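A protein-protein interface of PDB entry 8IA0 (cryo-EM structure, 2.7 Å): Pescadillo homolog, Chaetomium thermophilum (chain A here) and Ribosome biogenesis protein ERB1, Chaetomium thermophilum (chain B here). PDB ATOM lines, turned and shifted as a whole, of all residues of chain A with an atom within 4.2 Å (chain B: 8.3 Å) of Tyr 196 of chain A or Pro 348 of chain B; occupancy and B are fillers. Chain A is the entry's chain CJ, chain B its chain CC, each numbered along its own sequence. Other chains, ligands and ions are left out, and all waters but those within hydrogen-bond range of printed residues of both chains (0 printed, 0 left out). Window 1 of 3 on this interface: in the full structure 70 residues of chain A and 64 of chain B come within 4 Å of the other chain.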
ATOM      1  N   SER A 188     -23.421  21.020   5.658  1.00  0.00           N
ATOM      2  CA  SER A 188     -23.037  21.462   4.327  1.00  0.00           C
ATOM      3  C   SER A 188     -21.853  20.630   3.862  1.00  0.00           C
ATOM      4  O   SER A 188     -21.019  20.207   4.666  1.00  0.00           O
ATOM      5  CB  SER A 188     -22.688  22.952   4.299  1.00  0.00           C
ATOM      6  OG  SER A 188     -22.359  23.371   2.987  1.00  0.00           O
ATOM      7  N   PHE A 189     -21.783  20.401   2.554  1.00  0.00           N
ATOM      8  CA  PHE A 189     -20.817  19.461   2.006  1.00  0.00           C
ATOM      9  C   PHE A 189     -20.310  19.977   0.669  1.00  0.00           C
ATOM     10  O   PHE A 189     -21.090  20.456  -0.156  1.00  0.00           O
ATOM     11  CB  PHE A 189     -21.451  18.074   1.845  1.00  0.00           C
ATOM     12  CG  PHE A 189     -20.537  17.049   1.246  1.00  0.00           C
ATOM     13  CD1 PHE A 189     -19.258  16.868   1.736  1.00  0.00           C
ATOM     14  CD2 PHE A 189     -20.967  16.251   0.203  1.00  0.00           C
ATOM     15  CE1 PHE A 189     -18.422  15.920   1.188  1.00  0.00           C
ATOM     16  CE2 PHE A 189     -20.136  15.301  -0.346  1.00  0.00           C
ATOM     17  CZ  PHE A 189     -18.864  15.135   0.147  1.00  0.00           C
ATOM     18  N   SER A 191     -18.582  19.005  -2.845  1.00  0.00           N
ATOM     19  CA  SER A 191     -18.462  17.841  -3.706  1.00  0.00           C
ATOM     20  C   SER A 191     -17.994  18.278  -5.082  1.00  0.00           C
ATOM     21  O   SER A 191     -17.999  19.465  -5.416  1.00  0.00           O
ATOM     22  CB  SER A 191     -19.790  17.083  -3.817  1.00  0.00           C
ATOM     23  OG  SER A 191     -19.695  16.030  -4.759  1.00  0.00           O
ATOM     24  N   ILE A 195     -22.258  22.065  -4.144  1.00  0.00           N
ATOM     25  CA  ILE A 195     -22.334  22.233  -2.699  1.00  0.00           C
ATOM     26  C   ILE A 195     -23.685  21.725  -2.224  1.00  0.00           C
ATOM     27  O   ILE A 195     -24.726  22.115  -2.766  1.00  0.00           O
ATOM     28  CB  ILE A 195     -22.129  23.701  -2.282  1.00  0.00           C
ATOM     29  CG1 ILE A 195     -20.699  24.138  -2.587  1.00  0.00           C
ATOM     30  CG2 ILE A 195     -22.424  23.883  -0.807  1.00  0.00           C
ATOM     31  CD1 ILE A 195     -20.383  25.542  -2.147  1.00  0.00           C
ATOM     32  N   TYR A 196     -23.668  20.858  -1.218  1.00  0.00           N
ATOM     33  CA  TYR A 196     -24.878  20.286  -0.648  1.00  0.00           C
ATOM     34  C   TYR A 196     -25.217  21.006   0.649  1.00  0.00           C
ATOM     35  O   TYR A 196     -24.345  21.204   1.498  1.00  0.00           O
ATOM     36  CB  TYR A 196     -24.702  18.792  -0.382  1.00  0.00           C
ATOM     37  CG  TYR A 196     -24.792  17.919  -1.608  1.00  0.00           C
ATOM     38  CD1 TYR A 196     -26.014  17.440  -2.052  1.00  0.00           C
ATOM     39  CD2 TYR A 196     -23.654  17.557  -2.311  1.00  0.00           C
ATOM     40  CE1 TYR A 196     -26.101  16.634  -3.168  1.00  0.00           C
ATOM     41  CE2 TYR A 196     -23.731  16.753  -3.426  1.00  0.00           C
ATOM     42  CZ  TYR A 196     -24.956  16.293  -3.849  1.00  0.00           C
ATOM     43  OH  TYR A 196     -25.034  15.490  -4.962  1.00  0.00           O
ATOM     44  N   TYR A 197     -26.478  21.400   0.793  1.00  0.00           N
ATOM     45  CA  TYR A 197     -26.982  22.010   2.015  1.00  0.00           C
ATOM     46  C   TYR A 197     -28.088  21.138   2.586  1.00  0.00           C
ATOM     47  O   TYR A 197     -28.986  20.713   1.852  1.00  0.00           O
ATOM     48  CB  TYR A 197     -27.523  23.418   1.763  1.00  0.00           C
ATOM     49  CG  TYR A 197     -26.527  24.410   1.210  1.00  0.00           C
ATOM     50  CD1 TYR A 197     -25.601  25.028   2.035  1.00  0.00           C
ATOM     51  CD2 TYR A 197     -26.534  24.751  -0.134  1.00  0.00           C
ATOM     52  CE1 TYR A 197     -24.700  25.944   1.535  1.00  0.00           C
ATOM     53  CE2 TYR A 197     -25.637  25.666  -0.642  1.00  0.00           C
ATOM     54  CZ  TYR A 197     -24.723  26.260   0.197  1.00  0.00           C
ATOM     55  OH  TYR A 197     -23.827  27.170  -0.310  1.00  0.00           O
ATOM     56  N   LEU A 207     -32.567  18.449   1.807  1.00  0.00           N
ATOM     57  CA  LEU A 207     -31.255  18.415   1.178  1.00  0.00           C
ATOM     58  C   LEU A 207     -31.378  18.857  -0.270  1.00  0.00           C
ATOM     59  O   LEU A 207     -32.206  18.324  -1.017  1.00  0.00           O
ATOM     60  CB  LEU A 207     -30.649  17.013   1.253  1.00  0.00           C
ATOM     61  CG  LEU A 207     -29.238  16.854   0.690  1.00  0.00           C
ATOM     62  CD1 LEU A 207     -28.223  17.498   1.614  1.00  0.00           C
ATOM     63  CD2 LEU A 207     -28.912  15.387   0.473  1.00  0.00           C
ATOM     64  N   TRP A 208     -30.556  19.826  -0.667  1.00  0.00           N
ATOM     65  CA  TRP A 208     -30.547  20.310  -2.038  1.00  0.00           C
ATOM     66  C   TRP A 208     -29.120  20.621  -2.460  1.00  0.00           C
ATOM     67  O   TRP A 208     -28.246  20.883  -1.632  1.00  0.00           O
ATOM     68  CB  TRP A 208     -31.445  21.541  -2.217  1.00  0.00           C
ATOM     69  CG  TRP A 208     -30.975  22.774  -1.513  1.00  0.00           C
ATOM     70  CD1 TRP A 208     -30.300  23.821  -2.064  1.00  0.00           C
ATOM     71  CD2 TRP A 208     -31.175  23.107  -0.136  1.00  0.00           C
ATOM     72  NE1 TRP A 208     -30.053  24.778  -1.113  1.00  0.00           N
ATOM     73  CE2 TRP A 208     -30.583  24.365   0.080  1.00  0.00           C
ATOM     74  CE3 TRP A 208     -31.791  22.461   0.939  1.00  0.00           C
ATOM     75  CZ2 TRP A 208     -30.586  24.988   1.321  1.00  0.00           C
ATOM     76  CZ3 TRP A 208     -31.793  23.084   2.172  1.00  0.00           C
ATOM     77  CH2 TRP A 208     -31.195  24.333   2.353  1.00  0.00           C
ATOM     78  N   LEU A 209     -28.899  20.585  -3.770  1.00  0.00           N
ATOM     79  CA  LEU A 209     -27.580  20.747  -4.363  1.00  0.00           C
ATOM     80  C   LEU A 209     -27.541  22.028  -5.182  1.00  0.00           C
ATOM     81  O   LEU A 209     -28.455  22.293  -5.970  1.00  0.00           O
ATOM     82  CB  LEU A 209     -27.230  19.548  -5.244  1.00  0.00           C
ATOM     83  CG  LEU A 209     -25.920  19.630  -6.022  1.00  0.00           C
ATOM     84  CD1 LEU A 209     -24.744  19.803  -5.078  1.00  0.00           C
ATOM     85  CD2 LEU A 209     -25.738  18.397  -6.883  1.00  0.00           C
ATOM     86  N   SER A 487     -18.061  13.650   4.180  1.00  0.00           N
ATOM     87  CA  SER A 487     -19.476  13.930   3.978  1.00  0.00           C
ATOM     88  C   SER A 487     -20.249  13.682   5.265  1.00  0.00           C
ATOM     89  O   SER A 487     -20.168  12.580   5.821  1.00  0.00           O
ATOM     90  CB  SER A 487     -20.036  13.062   2.861  1.00  0.00           C
ATOM     91  OG  SER A 487     -20.246  11.735   3.308  1.00  0.00           O
ATOM     92  N   PHE A 489     -23.183  12.805   5.870  1.00  0.00           N
ATOM     93  CA  PHE A 489     -24.422  12.156   5.460  1.00  0.00           C
ATOM     94  C   PHE A 489     -24.397  10.639   5.550  1.00  0.00           C
ATOM     95  O   PHE A 489     -25.472  10.029   5.539  1.00  0.00           O
ATOM     96  CB  PHE A 489     -24.783  12.549   4.020  1.00  0.00           C
ATOM     97  CG  PHE A 489     -24.914  14.028   3.810  1.00  0.00           C
ATOM     98  CD1 PHE A 489     -25.788  14.775   4.578  1.00  0.00           C
ATOM     99  CD2 PHE A 489     -24.167  14.671   2.842  1.00  0.00           C
ATOM    100  CE1 PHE A 489     -25.911  16.134   4.386  1.00  0.00           C
ATOM    101  CE2 PHE A 489     -24.286  16.029   2.646  1.00  0.00           C
ATOM    102  CZ  PHE A 489     -25.158  16.761   3.419  1.00  0.00           C
ATOM    103  N   VAL A 490     -23.230  10.011   5.636  1.00  0.00           N
ATOM    104  CA  VAL A 490     -23.134   8.558   5.665  1.00  0.00           C
ATOM    105  C   VAL A 490     -23.221   8.095   7.112  1.00  0.00           C
ATOM    106  O   VAL A 490     -22.362   8.432   7.935  1.00  0.00           O
ATOM    107  CB  VAL A 490     -21.832   8.076   5.009  1.00  0.00           C
ATOM    108  CG1 VAL A 490     -21.560   6.623   5.369  1.00  0.00           C
ATOM    109  CG2 VAL A 490     -21.903   8.252   3.500  1.00  0.00           C
ATOM    110  N   LEU B 345     -33.414  10.636  -3.948  1.00  0.00           N
ATOM    111  CA  LEU B 345     -32.091  10.315  -4.456  1.00  0.00           C
ATOM    112  C   LEU B 345     -31.145  10.071  -3.282  1.00  0.00           C
ATOM    113  O   LEU B 345     -31.220  10.776  -2.269  1.00  0.00           O
ATOM    114  CB  LEU B 345     -31.565  11.445  -5.338  1.00  0.00           C
ATOM    115  CG  LEU B 345     -32.305  11.659  -6.659  1.00  0.00           C
ATOM    116  CD1 LEU B 345     -31.796  12.905  -7.367  1.00  0.00           C
ATOM    117  CD2 LEU B 345     -32.170  10.437  -7.555  1.00  0.00           C
ATOM    118  N   PRO B 346     -30.259   9.080  -3.375  1.00  0.00           N
ATOM    119  CA  PRO B 346     -29.452   8.718  -2.215  1.00  0.00           C
ATOM    120  C   PRO B 346     -28.542   9.861  -1.811  1.00  0.00           C
ATOM    121  O   PRO B 346     -28.096  10.654  -2.660  1.00  0.00           O
ATOM    122  CB  PRO B 346     -28.651   7.504  -2.708  1.00  0.00           C
ATOM    123  CG  PRO B 346     -29.401   6.997  -3.891  1.00  0.00           C
ATOM    124  CD  PRO B 346     -30.001   8.205  -4.527  1.00  0.00           C
ATOM    125  N   PRO B 347     -28.247   9.988  -0.517  1.00  0.00           N
ATOM    126  CA  PRO B 347     -27.380  11.075  -0.073  1.00  0.00           C
ATOM    127  C   PRO B 347     -25.965  10.878  -0.583  1.00  0.00           C
ATOM    128  O   PRO B 347     -25.548   9.744  -0.876  1.00  0.00           O
ATOM    129  CB  PRO B 347     -27.445  10.974   1.462  1.00  0.00           C
ATOM    130  CG  PRO B 347     -27.773   9.552   1.723  1.00  0.00           C
ATOM    131  CD  PRO B 347     -28.663   9.118   0.596  1.00  0.00           C
ATOM    132  N   PRO B 348     -25.192  11.951  -0.719  1.00  0.00           N
ATOM    133  CA  PRO B 348     -23.822  11.814  -1.222  1.00  0.00           C
ATOM    134  C   PRO B 348     -22.946  11.036  -0.254  1.00  0.00           C
ATOM    135  O   PRO B 348     -23.167  11.034   0.960  1.00  0.00           O
ATOM    136  CB  PRO B 348     -23.339  13.263  -1.357  1.00  0.00           C
ATOM    137  CG  PRO B 348     -24.561  14.108  -1.234  1.00  0.00           C
ATOM    138  CD  PRO B 348     -25.526  13.347  -0.403  1.00  0.00           C
ATOM    139  N   GLY B 349     -21.937  10.365  -0.811  1.00  0.00           N
ATOM    140  CA  GLY B 349     -21.011   9.576  -0.045  1.00  0.00           C
ATOM    141  C   GLY B 349     -19.656  10.236   0.095  1.00  0.00           C
ATOM    142  O   GLY B 349     -19.500  11.453  -0.074  1.00  0.00           O
ATOM    143  N   TYR B 350     -18.654   9.418   0.411  1.00  0.00           N
ATOM    144  CA  TYR B 350     -17.295   9.913   0.571  1.00  0.00           C
ATOM    145  C   TYR B 350     -16.527   9.975  -0.740  1.00  0.00           C
ATOM    146  O   TYR B 350     -15.449  10.576  -0.778  1.00  0.00           O
ATOM    147  CB  TYR B 350     -16.534   9.039   1.567  1.00  0.00           C
ATOM    148  CG  TYR B 350     -17.037   9.136   2.985  1.00  0.00           C
ATOM    149  CD1 TYR B 350     -17.000  10.337   3.674  1.00  0.00           C
ATOM    150  CD2 TYR B 350     -17.544   8.023   3.639  1.00  0.00           C
ATOM    151  CE1 TYR B 350     -17.458  10.430   4.972  1.00  0.00           C
ATOM    152  CE2 TYR B 350     -18.003   8.106   4.934  1.00  0.00           C
ATOM    153  CZ  TYR B 350     -17.958   9.312   5.596  1.00  0.00           C
ATOM    154  OH  TYR B 350     -18.415   9.398   6.889  1.00  0.00           O
ATOM    155  N   ASP B 351     -17.047   9.371  -1.810  1.00  0.00           N
ATOM    156  CA  ASP B 351     -16.376   9.453  -3.102  1.00  0.00           C
ATOM    157  C   ASP B 351     -16.569  10.815  -3.752  1.00  0.00           C
ATOM    158  O   ASP B 351     -15.764  11.217  -4.599  1.00  0.00           O
ATOM    159  CB  ASP B 351     -16.893   8.360  -4.036  1.00  0.00           C
ATOM    160  CG  ASP B 351     -17.197   7.066  -3.312  1.00  0.00           C
ATOM    161  OD1 ASP B 351     -18.252   6.990  -2.648  1.00  0.00           O
ATOM    162  OD2 ASP B 351     -16.389   6.120  -3.418  1.00  0.00           O
ATOM    163  N   LEU B 352     -17.622  11.534  -3.373  1.00  0.00           N
ATOM    164  CA  LEU B 352     -18.029  12.732  -4.094  1.00  0.00           C
ATOM    165  C   LEU B 352     -17.290  13.992  -3.665  1.00  0.00           C
ATOM    166  O   LEU B 352     -17.332  14.984  -4.398  1.00  0.00           O
ATOM    167  CB  LEU B 352     -19.534  12.941  -3.932  1.00  0.00           C
ATOM    168  CG  LEU B 352     -20.400  12.239  -4.976  1.00  0.00           C
ATOM    169  CD1 LEU B 352     -21.865  12.288  -4.585  1.00  0.00           C
ATOM    170  CD2 LEU B 352     -20.183  12.877  -6.334  1.00  0.00           C
ATOM    171  N   SER B 353     -16.613  13.983  -2.520  1.00  0.00           N
ATOM    172  CA  SER B 353     -15.979  15.195  -2.023  1.00  0.00           C
ATOM    173  C   SER B 353     -14.835  15.633  -2.930  1.00  0.00           C
ATOM    174  O   SER B 353     -14.169  14.815  -3.570  1.00  0.00           O
ATOM    175  CB  SER B 353     -15.468  14.983  -0.600  1.00  0.00           C
ATOM    176  OG  SER B 353     -14.577  13.887  -0.541  1.00  0.00           O
ATOM    177  N   TYR B 382     -19.595   9.090 -12.398  1.00  0.00           N
ATOM    178  CA  TYR B 382     -18.466   9.919 -12.008  1.00  0.00           C
ATOM    179  C   TYR B 382     -17.351   9.044 -11.461  1.00  0.00           C
ATOM    180  O   TYR B 382     -17.571   7.900 -11.053  1.00  0.00           O
ATOM    181  CB  TYR B 382     -18.885  10.977 -10.976  1.00  0.00           C
ATOM    182  CG  TYR B 382     -19.236  10.426  -9.611  1.00  0.00           C
ATOM    183  CD1 TYR B 382     -18.252  10.074  -8.698  1.00  0.00           C
ATOM    184  CD2 TYR B 382     -20.559  10.295  -9.222  1.00  0.00           C
ATOM    185  CE1 TYR B 382     -18.575   9.578  -7.456  1.00  0.00           C
ATOM    186  CE2 TYR B 382     -20.891   9.805  -7.978  1.00  0.00           C
ATOM    187  CZ  TYR B 382     -19.895   9.448  -7.100  1.00  0.00           C
ATOM    188  OH  TYR B 382     -20.219   8.958  -5.857  1.00  0.00           O
ATOM    189  N   PHE B 399     -24.341  18.671 -14.997  1.00  0.00           N
ATOM    190  CA  PHE B 399     -25.242  19.206 -13.982  1.00  0.00           C
ATOM    191  C   PHE B 399     -26.647  19.404 -14.537  1.00  0.00           C
ATOM    192  O   PHE B 399     -27.633  18.940 -13.952  1.00  0.00           O
ATOM    193  CB  PHE B 399     -24.698  20.519 -13.422  1.00  0.00           C
ATOM    194  CG  PHE B 399     -25.236  20.859 -12.065  1.00  0.00           C
ATOM    195  CD1 PHE B 399     -26.449  21.506 -11.928  1.00  0.00           C
ATOM    196  CD2 PHE B 399     -24.534  20.518 -10.926  1.00  0.00           C
ATOM    197  CE1 PHE B 399     -26.948  21.811 -10.681  1.00  0.00           C
ATOM    198  CE2 PHE B 399     -25.029  20.821  -9.679  1.00  0.00           C
ATOM    199  CZ  PHE B 399     -26.237  21.467  -9.557  1.00  0.00           C
ATOM    200  N   GLU B 402     -28.214  15.942 -15.702  1.00  0.00           N
ATOM    201  CA  GLU B 402     -28.728  15.102 -14.625  1.00  0.00           C
ATOM    202  C   GLU B 402     -30.062  15.620 -14.105  1.00  0.00           C
ATOM    203  O   GLU B 402     -30.978  14.834 -13.838  1.00  0.00           O
ATOM    204  CB  GLU B 402     -27.710  15.021 -13.488  1.00  0.00           C
ATOM    205  CG  GLU B 402     -26.531  14.106 -13.761  1.00  0.00           C
ATOM    206  CD  GLU B 402     -25.675  13.884 -12.530  1.00  0.00           C
ATOM    207  OE1 GLU B 402     -26.139  14.209 -11.417  1.00  0.00           O
ATOM    208  OE2 GLU B 402     -24.538  13.390 -12.675  1.00  0.00           O
ATOM    209  N   ARG B 403     -30.189  16.938 -13.950  1.00  0.00           N
ATOM    210  CA  ARG B 403     -31.432  17.507 -13.443  1.00  0.00           C
ATOM    211  C   ARG B 403     -32.563  17.333 -14.449  1.00  0.00           C
ATOM    212  O   ARG B 403     -33.718  17.118 -14.064  1.00  0.00           O
ATOM    213  CB  ARG B 403     -31.227  18.981 -13.095  1.00  0.00           C
ATOM    214  CG  ARG B 403     -32.491  19.745 -12.729  1.00  0.00           C
ATOM    215  CD  ARG B 403     -33.229  19.110 -11.561  1.00  0.00           C
ATOM    216  NE  ARG B 403     -32.321  18.582 -10.553  1.00  0.00           N
ATOM    217  CZ  ARG B 403     -32.700  18.142  -9.362  1.00  0.00           C
ATOM    218  NH1 ARG B 403     -33.968  18.157  -8.990  1.00  0.00           N
ATOM    219  NH2 ARG B 403     -31.782  17.671  -8.522  1.00  0.00           N
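Of chain B, only Pro 348 comes within 4 Å of Tyr 196 of chain A.
Of the printed residues of chain A, Gly 349 of chain B touches Phe 189, Ser 487 and Val 490.
Of the printed residues of chain A, Leu 352 of chain B touches Ser 191.
Of the printed residues of chain B, Leu 209 of chain A touches Phe 399.
Of the printed residues of chain A, Ser 353 of chain B touches Phe 189 (3.5 Å) and Ser 191 (3.9999 Å).
Of the printed residues of chain B, Phe 189 of chain A touches Pro 348, Gly 349 and Ser 353.
The nearest residue of chain B that does not touch Tyr 196 of chain A is Leu 352 of chain B (4.5 Å).
The nearest residue of chain A that does not touch Pro 348 of chain B is Leu 207 of chain A (4.05 Å).
The nearest printed residue of chain A that does not touch Gly 349 of chain B is Phe 489 of chain A (6.0 Å).
OG of Ser 188 of chain A sits close to O of Tyr 196 of chain A, at 3.3 Å.
O of Phe 189 of chain A lies within hydrogen-bond range of N of Tyr 196 of chain A, at 2.8 Å.
O of Tyr 350 of chain B is in hydrogen-bond range of OG of Ser 353 of chain B (3.4 Å).
OG of Ser 191 of chain A is in hydrogen-bond range of O of Leu 352 of chain B (2.6 Å).
OG of Ser 487 of chain A sits close to O of Gly 349 of chain B (3.5 Å).
CB of Pro 348 of chain B touches CE2 of Phe 189 of chain A (3.9 Å).
Phe 189 of chain A touches Gly 349 of chain B.
Ser 353 of chain B touches Phe 189 of chain A (CB to CZ, 3.5 Å).
Ser 353 of chain B touches Ser 191 of chain A.
Phe 399 of chain B touches Leu 209 of chain A (CE2 to CD2, 3.8 Å).
CE1 of Tyr 350 of chain B touches N of Ser 487 of chain A (3.4 Å).
Phe 489 of chain A touches Pro 348 of chain B.
Pro 348 of chain B touches Val 490 of chain A (O to CG2, 3.97 Å).
Val 490 of chain A touches Gly 349 of chain B.
Val 490 of chain A touches Tyr 350 of chain B (CB to CE2, 3.8 Å).
Of the 12 printed residues of chain A, 7 touch a printed residue of chain B.
Printed residues of chain B that touch a printed residue of chain A: Pro 348, Gly 349, Tyr 350, Leu 352, Ser 353 and Phe 399.
Along chain B the printed residues that touch a printed residue of chain A span positions 348 to 399.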
